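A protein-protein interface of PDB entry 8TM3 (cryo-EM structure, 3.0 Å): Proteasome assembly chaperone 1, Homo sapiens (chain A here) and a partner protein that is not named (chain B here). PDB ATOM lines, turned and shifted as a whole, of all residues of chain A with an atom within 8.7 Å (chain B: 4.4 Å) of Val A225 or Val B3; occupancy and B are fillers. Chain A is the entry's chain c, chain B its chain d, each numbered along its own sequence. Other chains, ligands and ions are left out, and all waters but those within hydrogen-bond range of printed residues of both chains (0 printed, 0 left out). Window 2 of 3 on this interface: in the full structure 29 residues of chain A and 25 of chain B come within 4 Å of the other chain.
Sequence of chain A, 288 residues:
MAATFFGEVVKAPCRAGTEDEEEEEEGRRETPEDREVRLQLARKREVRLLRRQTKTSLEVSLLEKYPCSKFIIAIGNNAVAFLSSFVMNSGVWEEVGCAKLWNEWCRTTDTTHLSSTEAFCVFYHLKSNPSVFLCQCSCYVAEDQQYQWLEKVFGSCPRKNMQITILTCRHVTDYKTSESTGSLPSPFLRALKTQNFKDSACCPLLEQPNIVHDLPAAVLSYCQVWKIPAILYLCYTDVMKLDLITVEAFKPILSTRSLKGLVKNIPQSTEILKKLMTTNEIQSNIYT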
ATOM      1  N   TYR A 147       4.398 -13.053 -24.863  1.00  0.00           N
ATOM      2  CA  TYR A 147       5.347 -13.913 -25.562  1.00  0.00           C
ATOM      3  C   TYR A 147       6.762 -13.732 -25.028  1.00  0.00           C
ATOM      4  O   TYR A 147       7.545 -14.688 -25.015  1.00  0.00           O
ATOM      5  CB  TYR A 147       5.281 -13.632 -27.064  1.00  0.00           C
ATOM      6  CG  TYR A 147       4.068 -14.231 -27.759  1.00  0.00           C
ATOM      7  CD1 TYR A 147       3.358 -15.288 -27.196  1.00  0.00           C
ATOM      8  CD2 TYR A 147       3.641 -13.746 -28.986  1.00  0.00           C
ATOM      9  CE1 TYR A 147       2.258 -15.831 -27.829  1.00  0.00           C
ATOM     10  CE2 TYR A 147       2.535 -14.284 -29.623  1.00  0.00           C
ATOM     11  CZ  TYR A 147       1.853 -15.327 -29.042  1.00  0.00           C
ATOM     12  OH  TYR A 147       0.758 -15.867 -29.676  1.00  0.00           O
ATOM     13  N   PRO A 158      12.266 -26.642 -25.132  1.00  0.00           N
ATOM     14  CA  PRO A 158      11.346 -27.275 -24.183  1.00  0.00           C
ATOM     15  C   PRO A 158      11.675 -28.750 -23.977  1.00  0.00           C
ATOM     16  O   PRO A 158      12.419 -29.369 -24.739  1.00  0.00           O
ATOM     17  CB  PRO A 158       9.979 -27.095 -24.846  1.00  0.00           C
ATOM     18  CG  PRO A 158      10.273 -27.049 -26.303  1.00  0.00           C
ATOM     19  CD  PRO A 158      11.655 -26.466 -26.461  1.00  0.00           C
ATOM     20  N   THR A 194      -5.277 -29.968 -24.210  1.00  0.00           N
ATOM     21  CA  THR A 194      -4.552 -29.916 -25.469  1.00  0.00           C
ATOM     22  C   THR A 194      -4.661 -31.258 -26.188  1.00  0.00           C
ATOM     23  O   THR A 194      -5.368 -32.173 -25.758  1.00  0.00           O
ATOM     24  CB  THR A 194      -3.088 -29.530 -25.236  1.00  0.00           C
ATOM     25  OG1 THR A 194      -2.483 -29.168 -26.484  1.00  0.00           O
ATOM     26  CG2 THR A 194      -2.313 -30.681 -24.619  1.00  0.00           C
ATOM     27  N   GLN A 195      -3.945 -31.372 -27.309  1.00  0.00           N
ATOM     28  CA  GLN A 195      -4.076 -32.552 -28.158  1.00  0.00           C
ATOM     29  C   GLN A 195      -3.588 -33.809 -27.448  1.00  0.00           C
ATOM     30  O   GLN A 195      -4.261 -34.846 -27.469  1.00  0.00           O
ATOM     31  CB  GLN A 195      -3.306 -32.340 -29.462  1.00  0.00           C
ATOM     32  N   ASN A 196      -2.420 -33.737 -26.809  1.00  0.00           N
ATOM     33  CA  ASN A 196      -1.761 -34.908 -26.243  1.00  0.00           C
ATOM     34  C   ASN A 196      -1.827 -34.933 -24.718  1.00  0.00           C
ATOM     35  O   ASN A 196      -0.942 -35.488 -24.063  1.00  0.00           O
ATOM     36  CB  ASN A 196      -0.308 -34.971 -26.710  1.00  0.00           C
ATOM     37  CG  ASN A 196       0.472 -33.722 -26.360  1.00  0.00           C
ATOM     38  OD1 ASN A 196      -0.073 -32.619 -26.356  1.00  0.00           O
ATOM     39  ND2 ASN A 196       1.755 -33.887 -26.066  1.00  0.00           N
ATOM     40  N   ALA A 217      -3.979 -18.297 -22.323  1.00  0.00           N
ATOM     41  CA  ALA A 217      -4.049 -18.682 -23.724  1.00  0.00           C
ATOM     42  C   ALA A 217      -2.666 -18.720 -24.355  1.00  0.00           C
ATOM     43  O   ALA A 217      -2.396 -19.585 -25.191  1.00  0.00           O
ATOM     44  CB  ALA A 217      -4.955 -17.720 -24.488  1.00  0.00           C
ATOM     45  N   ALA A 218      -1.781 -17.798 -23.974  1.00  0.00           N
ATOM     46  CA  ALA A 218      -0.426 -17.805 -24.517  1.00  0.00           C
ATOM     47  C   ALA A 218       0.287 -19.108 -24.183  1.00  0.00           C
ATOM     48  O   ALA A 218       0.864 -19.764 -25.061  1.00  0.00           O
ATOM     49  CB  ALA A 218       0.359 -16.612 -23.972  1.00  0.00           C
ATOM     50  N   VAL A 219       0.253 -19.502 -22.910  1.00  0.00           N
ATOM     51  CA  VAL A 219       0.943 -20.721 -22.501  1.00  0.00           C
ATOM     52  C   VAL A 219       0.293 -21.941 -23.139  1.00  0.00           C
ATOM     53  O   VAL A 219       0.984 -22.877 -23.559  1.00  0.00           O
ATOM     54  CB  VAL A 219       0.975 -20.839 -20.966  1.00  0.00           C
ATOM     55  CG1 VAL A 219       1.896 -21.975 -20.550  1.00  0.00           C
ATOM     56  CG2 VAL A 219       1.442 -19.539 -20.333  1.00  0.00           C
ATOM     57  N   LEU A 220      -1.040 -21.961 -23.219  1.00  0.00           N
ATOM     58  CA  LEU A 220      -1.708 -23.103 -23.834  1.00  0.00           C
ATOM     59  C   LEU A 220      -1.366 -23.209 -25.316  1.00  0.00           C
ATOM     60  O   LEU A 220      -1.173 -24.313 -25.836  1.00  0.00           O
ATOM     61  CB  LEU A 220      -3.218 -22.998 -23.632  1.00  0.00           C
ATOM     62  CG  LEU A 220      -3.962 -24.334 -23.626  1.00  0.00           C
ATOM     63  CD1 LEU A 220      -3.642 -25.121 -22.366  1.00  0.00           C
ATOM     64  CD2 LEU A 220      -5.458 -24.115 -23.751  1.00  0.00           C
ATOM     65  N   SER A 221      -1.289 -22.077 -26.016  1.00  0.00           N
ATOM     66  CA  SER A 221      -0.894 -22.102 -27.418  1.00  0.00           C
ATOM     67  C   SER A 221       0.539 -22.593 -27.572  1.00  0.00           C
ATOM     68  O   SER A 221       0.838 -23.385 -28.474  1.00  0.00           O
ATOM     69  CB  SER A 221      -1.054 -20.712 -28.034  1.00  0.00           C
ATOM     70  OG  SER A 221       0.185 -20.024 -28.072  1.00  0.00           O
ATOM     71  N   TYR A 222       1.439 -22.135 -26.700  1.00  0.00           N
ATOM     72  CA  TYR A 222       2.815 -22.617 -26.751  1.00  0.00           C
ATOM     73  C   TYR A 222       2.864 -24.126 -26.560  1.00  0.00           C
ATOM     74  O   TYR A 222       3.567 -24.836 -27.289  1.00  0.00           O
ATOM     75  CB  TYR A 222       3.657 -21.912 -25.688  1.00  0.00           C
ATOM     76  CG  TYR A 222       5.090 -22.394 -25.612  1.00  0.00           C
ATOM     77  CD1 TYR A 222       5.420 -23.555 -24.923  1.00  0.00           C
ATOM     78  CD2 TYR A 222       6.115 -21.685 -26.224  1.00  0.00           C
ATOM     79  CE1 TYR A 222       6.726 -23.997 -24.850  1.00  0.00           C
ATOM     80  CE2 TYR A 222       7.425 -22.120 -26.156  1.00  0.00           C
ATOM     81  CZ  TYR A 222       7.724 -23.276 -25.467  1.00  0.00           C
ATOM     82  OH  TYR A 222       9.027 -23.713 -25.397  1.00  0.00           O
ATOM     83  N   CYS A 223       2.118 -24.634 -25.579  1.00  0.00           N
ATOM     84  CA  CYS A 223       2.110 -26.071 -25.326  1.00  0.00           C
ATOM     85  C   CYS A 223       1.556 -26.838 -26.519  1.00  0.00           C
ATOM     86  O   CYS A 223       2.121 -27.859 -26.927  1.00  0.00           O
ATOM     87  CB  CYS A 223       1.290 -26.371 -24.074  1.00  0.00           C
ATOM     88  SG  CYS A 223      -0.452 -26.679 -24.413  1.00  0.00           S
ATOM     89  N   GLN A 224       0.449 -26.360 -27.091  1.00  0.00           N
ATOM     90  CA  GLN A 224      -0.159 -27.053 -28.222  1.00  0.00           C
ATOM     91  C   GLN A 224       0.776 -27.071 -29.424  1.00  0.00           C
ATOM     92  O   GLN A 224       0.915 -28.099 -30.097  1.00  0.00           O
ATOM     93  CB  GLN A 224      -1.485 -26.385 -28.585  1.00  0.00           C
ATOM     94  CG  GLN A 224      -2.183 -26.975 -29.801  1.00  0.00           C
ATOM     95  CD  GLN A 224      -2.569 -28.425 -29.605  1.00  0.00           C
ATOM     96  OE1 GLN A 224      -3.214 -28.780 -28.619  1.00  0.00           O
ATOM     97  NE2 GLN A 224      -2.175 -29.274 -30.546  1.00  0.00           N
ATOM     98  N   VAL A 225       1.427 -25.942 -29.707  1.00  0.00           N
ATOM     99  CA  VAL A 225       2.292 -25.859 -30.879  1.00  0.00           C
ATOM    100  C   VAL A 225       3.458 -26.830 -30.754  1.00  0.00           C
ATOM    101  O   VAL A 225       3.815 -27.522 -31.715  1.00  0.00           O
ATOM    102  CB  VAL A 225       2.778 -24.412 -31.075  1.00  0.00           C
ATOM    103  CG1 VAL A 225       3.906 -24.359 -32.092  1.00  0.00           C
ATOM    104  CG2 VAL A 225       1.623 -23.525 -31.506  1.00  0.00           C
ATOM    105  N   TRP A 226       4.066 -26.902 -29.572  1.00  0.00           N
ATOM    106  CA  TRP A 226       5.226 -27.749 -29.341  1.00  0.00           C
ATOM    107  C   TRP A 226       4.852 -29.112 -28.773  1.00  0.00           C
ATOM    108  O   TRP A 226       5.738 -29.861 -28.352  1.00  0.00           O
ATOM    109  CB  TRP A 226       6.212 -27.041 -28.412  1.00  0.00           C
ATOM    110  CG  TRP A 226       6.771 -25.777 -28.995  1.00  0.00           C
ATOM    111  CD1 TRP A 226       6.788 -24.545 -28.413  1.00  0.00           C
ATOM    112  CD2 TRP A 226       7.394 -25.621 -30.277  1.00  0.00           C
ATOM    113  NE1 TRP A 226       7.381 -23.631 -29.250  1.00  0.00           N
ATOM    114  CE2 TRP A 226       7.763 -24.267 -30.401  1.00  0.00           C
ATOM    115  CE3 TRP A 226       7.676 -26.495 -31.331  1.00  0.00           C
ATOM    116  CZ2 TRP A 226       8.397 -23.767 -31.535  1.00  0.00           C
ATOM    117  CZ3 TRP A 226       8.307 -25.996 -32.457  1.00  0.00           C
ATOM    118  CH2 TRP A 226       8.660 -24.645 -32.549  1.00  0.00           C
ATOM    119  N   LYS A 227       3.562 -29.449 -28.751  1.00  0.00           N
ATOM    120  CA  LYS A 227       3.098 -30.772 -28.338  1.00  0.00           C
ATOM    121  C   LYS A 227       3.534 -31.084 -26.905  1.00  0.00           C
ATOM    122  O   LYS A 227       4.302 -32.013 -26.643  1.00  0.00           O
ATOM    123  CB  LYS A 227       3.597 -31.844 -29.311  1.00  0.00           C
ATOM    124  N   ILE A 228       3.028 -30.283 -25.976  1.00  0.00           N
ATOM    125  CA  ILE A 228       3.263 -30.461 -24.550  1.00  0.00           C
ATOM    126  C   ILE A 228       1.913 -30.740 -23.898  1.00  0.00           C
ATOM    127  O   ILE A 228       0.994 -29.926 -24.018  1.00  0.00           O
ATOM    128  CB  ILE A 228       3.929 -29.228 -23.918  1.00  0.00           C
ATOM    129  CG1 ILE A 228       5.253 -28.928 -24.627  1.00  0.00           C
ATOM    130  CG2 ILE A 228       4.151 -29.443 -22.422  1.00  0.00           C
ATOM    131  CD1 ILE A 228       6.167 -27.981 -23.875  1.00  0.00           C
ATOM    132  N   MET B   1       7.033 -20.084 -39.822  1.00  0.00           N
ATOM    133  CA  MET B   1       6.663 -20.503 -38.441  1.00  0.00           C
ATOM    134  C   MET B   1       5.595 -21.588 -38.477  1.00  0.00           C
ATOM    135  O   MET B   1       4.806 -21.727 -37.543  1.00  0.00           O
ATOM    136  CB  MET B   1       6.165 -19.303 -37.634  1.00  0.00           C
ATOM    137  N   PHE B   2       5.574 -22.357 -39.562  1.00  0.00           N
ATOM    138  CA  PHE B   2       4.595 -23.425 -39.713  1.00  0.00           C
ATOM    139  C   PHE B   2       5.007 -24.628 -38.874  1.00  0.00           C
ATOM    140  O   PHE B   2       6.105 -25.167 -39.046  1.00  0.00           O
ATOM    141  CB  PHE B   2       4.466 -23.816 -41.183  1.00  0.00           C
ATOM    142  CG  PHE B   2       3.586 -25.008 -41.417  1.00  0.00           C
ATOM    143  CD1 PHE B   2       2.219 -24.856 -41.573  1.00  0.00           C
ATOM    144  CD2 PHE B   2       4.124 -26.280 -41.480  1.00  0.00           C
ATOM    145  CE1 PHE B   2       1.407 -25.952 -41.790  1.00  0.00           C
ATOM    146  CE2 PHE B   2       3.317 -27.380 -41.695  1.00  0.00           C
ATOM    147  CZ  PHE B   2       1.956 -27.215 -41.850  1.00  0.00           C
ATOM    148  N   VAL B   3       4.127 -25.047 -37.971  1.00  0.00           N
ATOM    149  CA  VAL B   3       4.369 -26.216 -37.130  1.00  0.00           C
ATOM    150  C   VAL B   3       3.318 -27.270 -37.461  1.00  0.00           C
ATOM    151  O   VAL B   3       2.125 -27.047 -37.211  1.00  0.00           O
ATOM    152  CB  VAL B   3       4.340 -25.846 -35.639  1.00  0.00           C
ATOM    153  CG1 VAL B   3       4.560 -27.080 -34.779  1.00  0.00           C
ATOM    154  CG2 VAL B   3       5.391 -24.787 -35.339  1.00  0.00           C
ATOM    155  N   PRO B   4       3.698 -28.420 -38.019  1.00  0.00           N
ATOM    156  CA  PRO B   4       2.688 -29.406 -38.418  1.00  0.00           C
ATOM    157  C   PRO B   4       1.928 -29.956 -37.221  1.00  0.00           C
ATOM    158  O   PRO B   4       2.454 -30.054 -36.111  1.00  0.00           O
ATOM    159  CB  PRO B   4       3.511 -30.501 -39.107  1.00  0.00           C
ATOM    160  CG  PRO B   4       4.885 -30.348 -38.566  1.00  0.00           C
ATOM    161  CD  PRO B   4       5.066 -28.886 -38.308  1.00  0.00           C
ATOM    162  N   CYS B   5       0.667 -30.319 -37.464  1.00  0.00           N
ATOM    163  CA  CYS B   5      -0.140 -30.925 -36.409  1.00  0.00           C
ATOM    164  C   CYS B   5       0.461 -32.250 -35.960  1.00  0.00           C
ATOM    165  O   CYS B   5       0.519 -32.540 -34.760  1.00  0.00           O
ATOM    166  CB  CYS B   5      -1.575 -31.124 -36.895  1.00  0.00           C
ATOM    167  N   GLY B  45      -1.509 -27.999 -39.719  1.00  0.00           N
ATOM    168  CA  GLY B  45      -0.396 -27.431 -38.991  1.00  0.00           C
ATOM    169  C   GLY B  45      -0.834 -26.283 -38.113  1.00  0.00           C
ATOM    170  O   GLY B  45      -2.026 -26.036 -37.923  1.00  0.00           O
ATOM    171  N   TYR B  46       0.161 -25.582 -37.575  1.00  0.00           N
ATOM    172  CA  TYR B  46      -0.066 -24.472 -36.654  1.00  0.00           C
ATOM    173  C   TYR B  46       0.982 -23.406 -36.932  1.00  0.00           C
ATOM    174  O   TYR B  46       2.153 -23.579 -36.582  1.00  0.00           O
ATOM    175  CB  TYR B  46       0.001 -24.945 -35.202  1.00  0.00           C
ATOM    176  CG  TYR B  46      -1.201 -25.757 -34.774  1.00  0.00           C
ATOM    177  CD1 TYR B  46      -2.487 -25.252 -34.907  1.00  0.00           C
ATOM    178  CD2 TYR B  46      -1.050 -27.032 -34.248  1.00  0.00           C
ATOM    179  CE1 TYR B  46      -3.587 -25.991 -34.522  1.00  0.00           C
ATOM    180  CE2 TYR B  46      -2.146 -27.779 -33.860  1.00  0.00           C
ATOM    181  CZ  TYR B  46      -3.412 -27.253 -33.999  1.00  0.00           C
ATOM    182  OH  TYR B  46      -4.509 -27.991 -33.615  1.00  0.00           O
ATOM    183  N   TYR B  48       2.632 -20.668 -35.812  1.00  0.00           N
ATOM    184  CA  TYR B  48       2.858 -19.998 -34.533  1.00  0.00           C
ATOM    185  C   TYR B  48       3.809 -18.830 -34.759  1.00  0.00           C
ATOM    186  O   TYR B  48       5.013 -19.021 -34.948  1.00  0.00           O
ATOM    187  CB  TYR B  48       3.413 -20.977 -33.504  1.00  0.00           C
ATOM    188  CG  TYR B  48       3.463 -20.428 -32.094  1.00  0.00           C
ATOM    189  CD1 TYR B  48       2.354 -19.816 -31.526  1.00  0.00           C
ATOM    190  CD2 TYR B  48       4.618 -20.528 -31.331  1.00  0.00           C
ATOM    191  CE1 TYR B  48       2.395 -19.315 -30.238  1.00  0.00           C
ATOM    192  CE2 TYR B  48       4.668 -20.029 -30.042  1.00  0.00           C
ATOM    193  CZ  TYR B  48       3.553 -19.425 -29.502  1.00  0.00           C
ATOM    194  OH  TYR B  48       3.596 -18.927 -28.220  1.00  0.00           O
ATOM    195  N   ILE B  73      -5.756 -22.395 -31.851  1.00  0.00           N
ATOM    196  CA  ILE B  73      -4.892 -21.279 -31.478  1.00  0.00           C
ATOM    197  C   ILE B  73      -5.169 -20.089 -32.387  1.00  0.00           C
ATOM    198  O   ILE B  73      -5.894 -20.205 -33.380  1.00  0.00           O
ATOM    199  CB  ILE B  73      -3.404 -21.670 -31.531  1.00  0.00           C
ATOM    200  CG1 ILE B  73      -3.023 -22.158 -32.930  1.00  0.00           C
ATOM    201  CG2 ILE B  73      -3.104 -22.732 -30.484  1.00  0.00           C
ATOM    202  CD1 ILE B  73      -1.605 -22.652 -33.033  1.00  0.00           C
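The backbone carbonyl oxygen (O) of Val B3 lies within hydrogen-bond range of the backbone NH (N) of Tyr B46. The backbone carbonyl oxygen (O) of Ala A218 sits at hydrogen-bond distance from the side-chain hydroxyl (OG) of Ser A221, at 3.1 Å. O of Met B1 lies within hydrogen-bond range of N of Tyr B48 (3.0 Å). N of Gln A195 lies within hydrogen-bond range of OE1 of Gln A224, at 3.0 Å.
Of the 9 printed residues of chain B, 4 touch a printed residue of chain A. Printed residues of chain B that touch a printed residue of chain A: Val B3, Tyr B46, Tyr B48 and Ile B73. Hydrophobic or aromatic side chains of chain B that line the printed part of chain A: Val B3, Tyr B46, Tyr B48 and Ile B73. Along chain B the printed residues that touch a printed residue of chain A span positions 3 to 73. Printed residues of chain A that touch a printed residue of chain B: Tyr A147, Ser A221, Tyr A222, Gln A224 and Val A225. Among the printed residues, 8 pairs touch across the chains. Among the printed residues, no Asp or Glu carboxylate lies within 4 Å of a Lys or Arg side-chain nitrogen of the other chain.
Of the printed residues of chain B, Val A225 touches Val B3, Tyr B48 and Ile B73. Of chain A, only Val A225 comes within 4 Å of Val B3. No residue of chain A comes within 4 Å of Pro B4. No residue of chain A comes within 4 Å of Gly B45. Of the printed residues of chain A, Tyr B48 touches Tyr A147, Ser A221, Tyr A222 and Val A225. Of the printed residues of chain A, Ile B73 touches Ser A221 and Val A225. Printed residues of chain B within 4 Å of Gln A224: Tyr B46. Lys A227 touches none of the printed residues of chain B. Leu A220 touches none of the printed residues of chain B. The nearest residue of chain A that does not touch Val B3 is Trp A226 (4.3 Å).
Among the printed residues, pairs that only touch across the chains: Tyr A147 with Tyr B48 (3.4 Å), Ser A221 with Tyr B48 (3.2 Å), Ser A221 with Ile B73 (3.8 Å), Tyr A222 with Tyr B48 (3.9 Å), Gln A224 with Tyr B46 (3.6 Å), Val A225 with Val B3 (3.2 Å), Val A225 with Tyr B48 (3.7 Å) and Val A225 with Ile B73 (3.7 Å).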
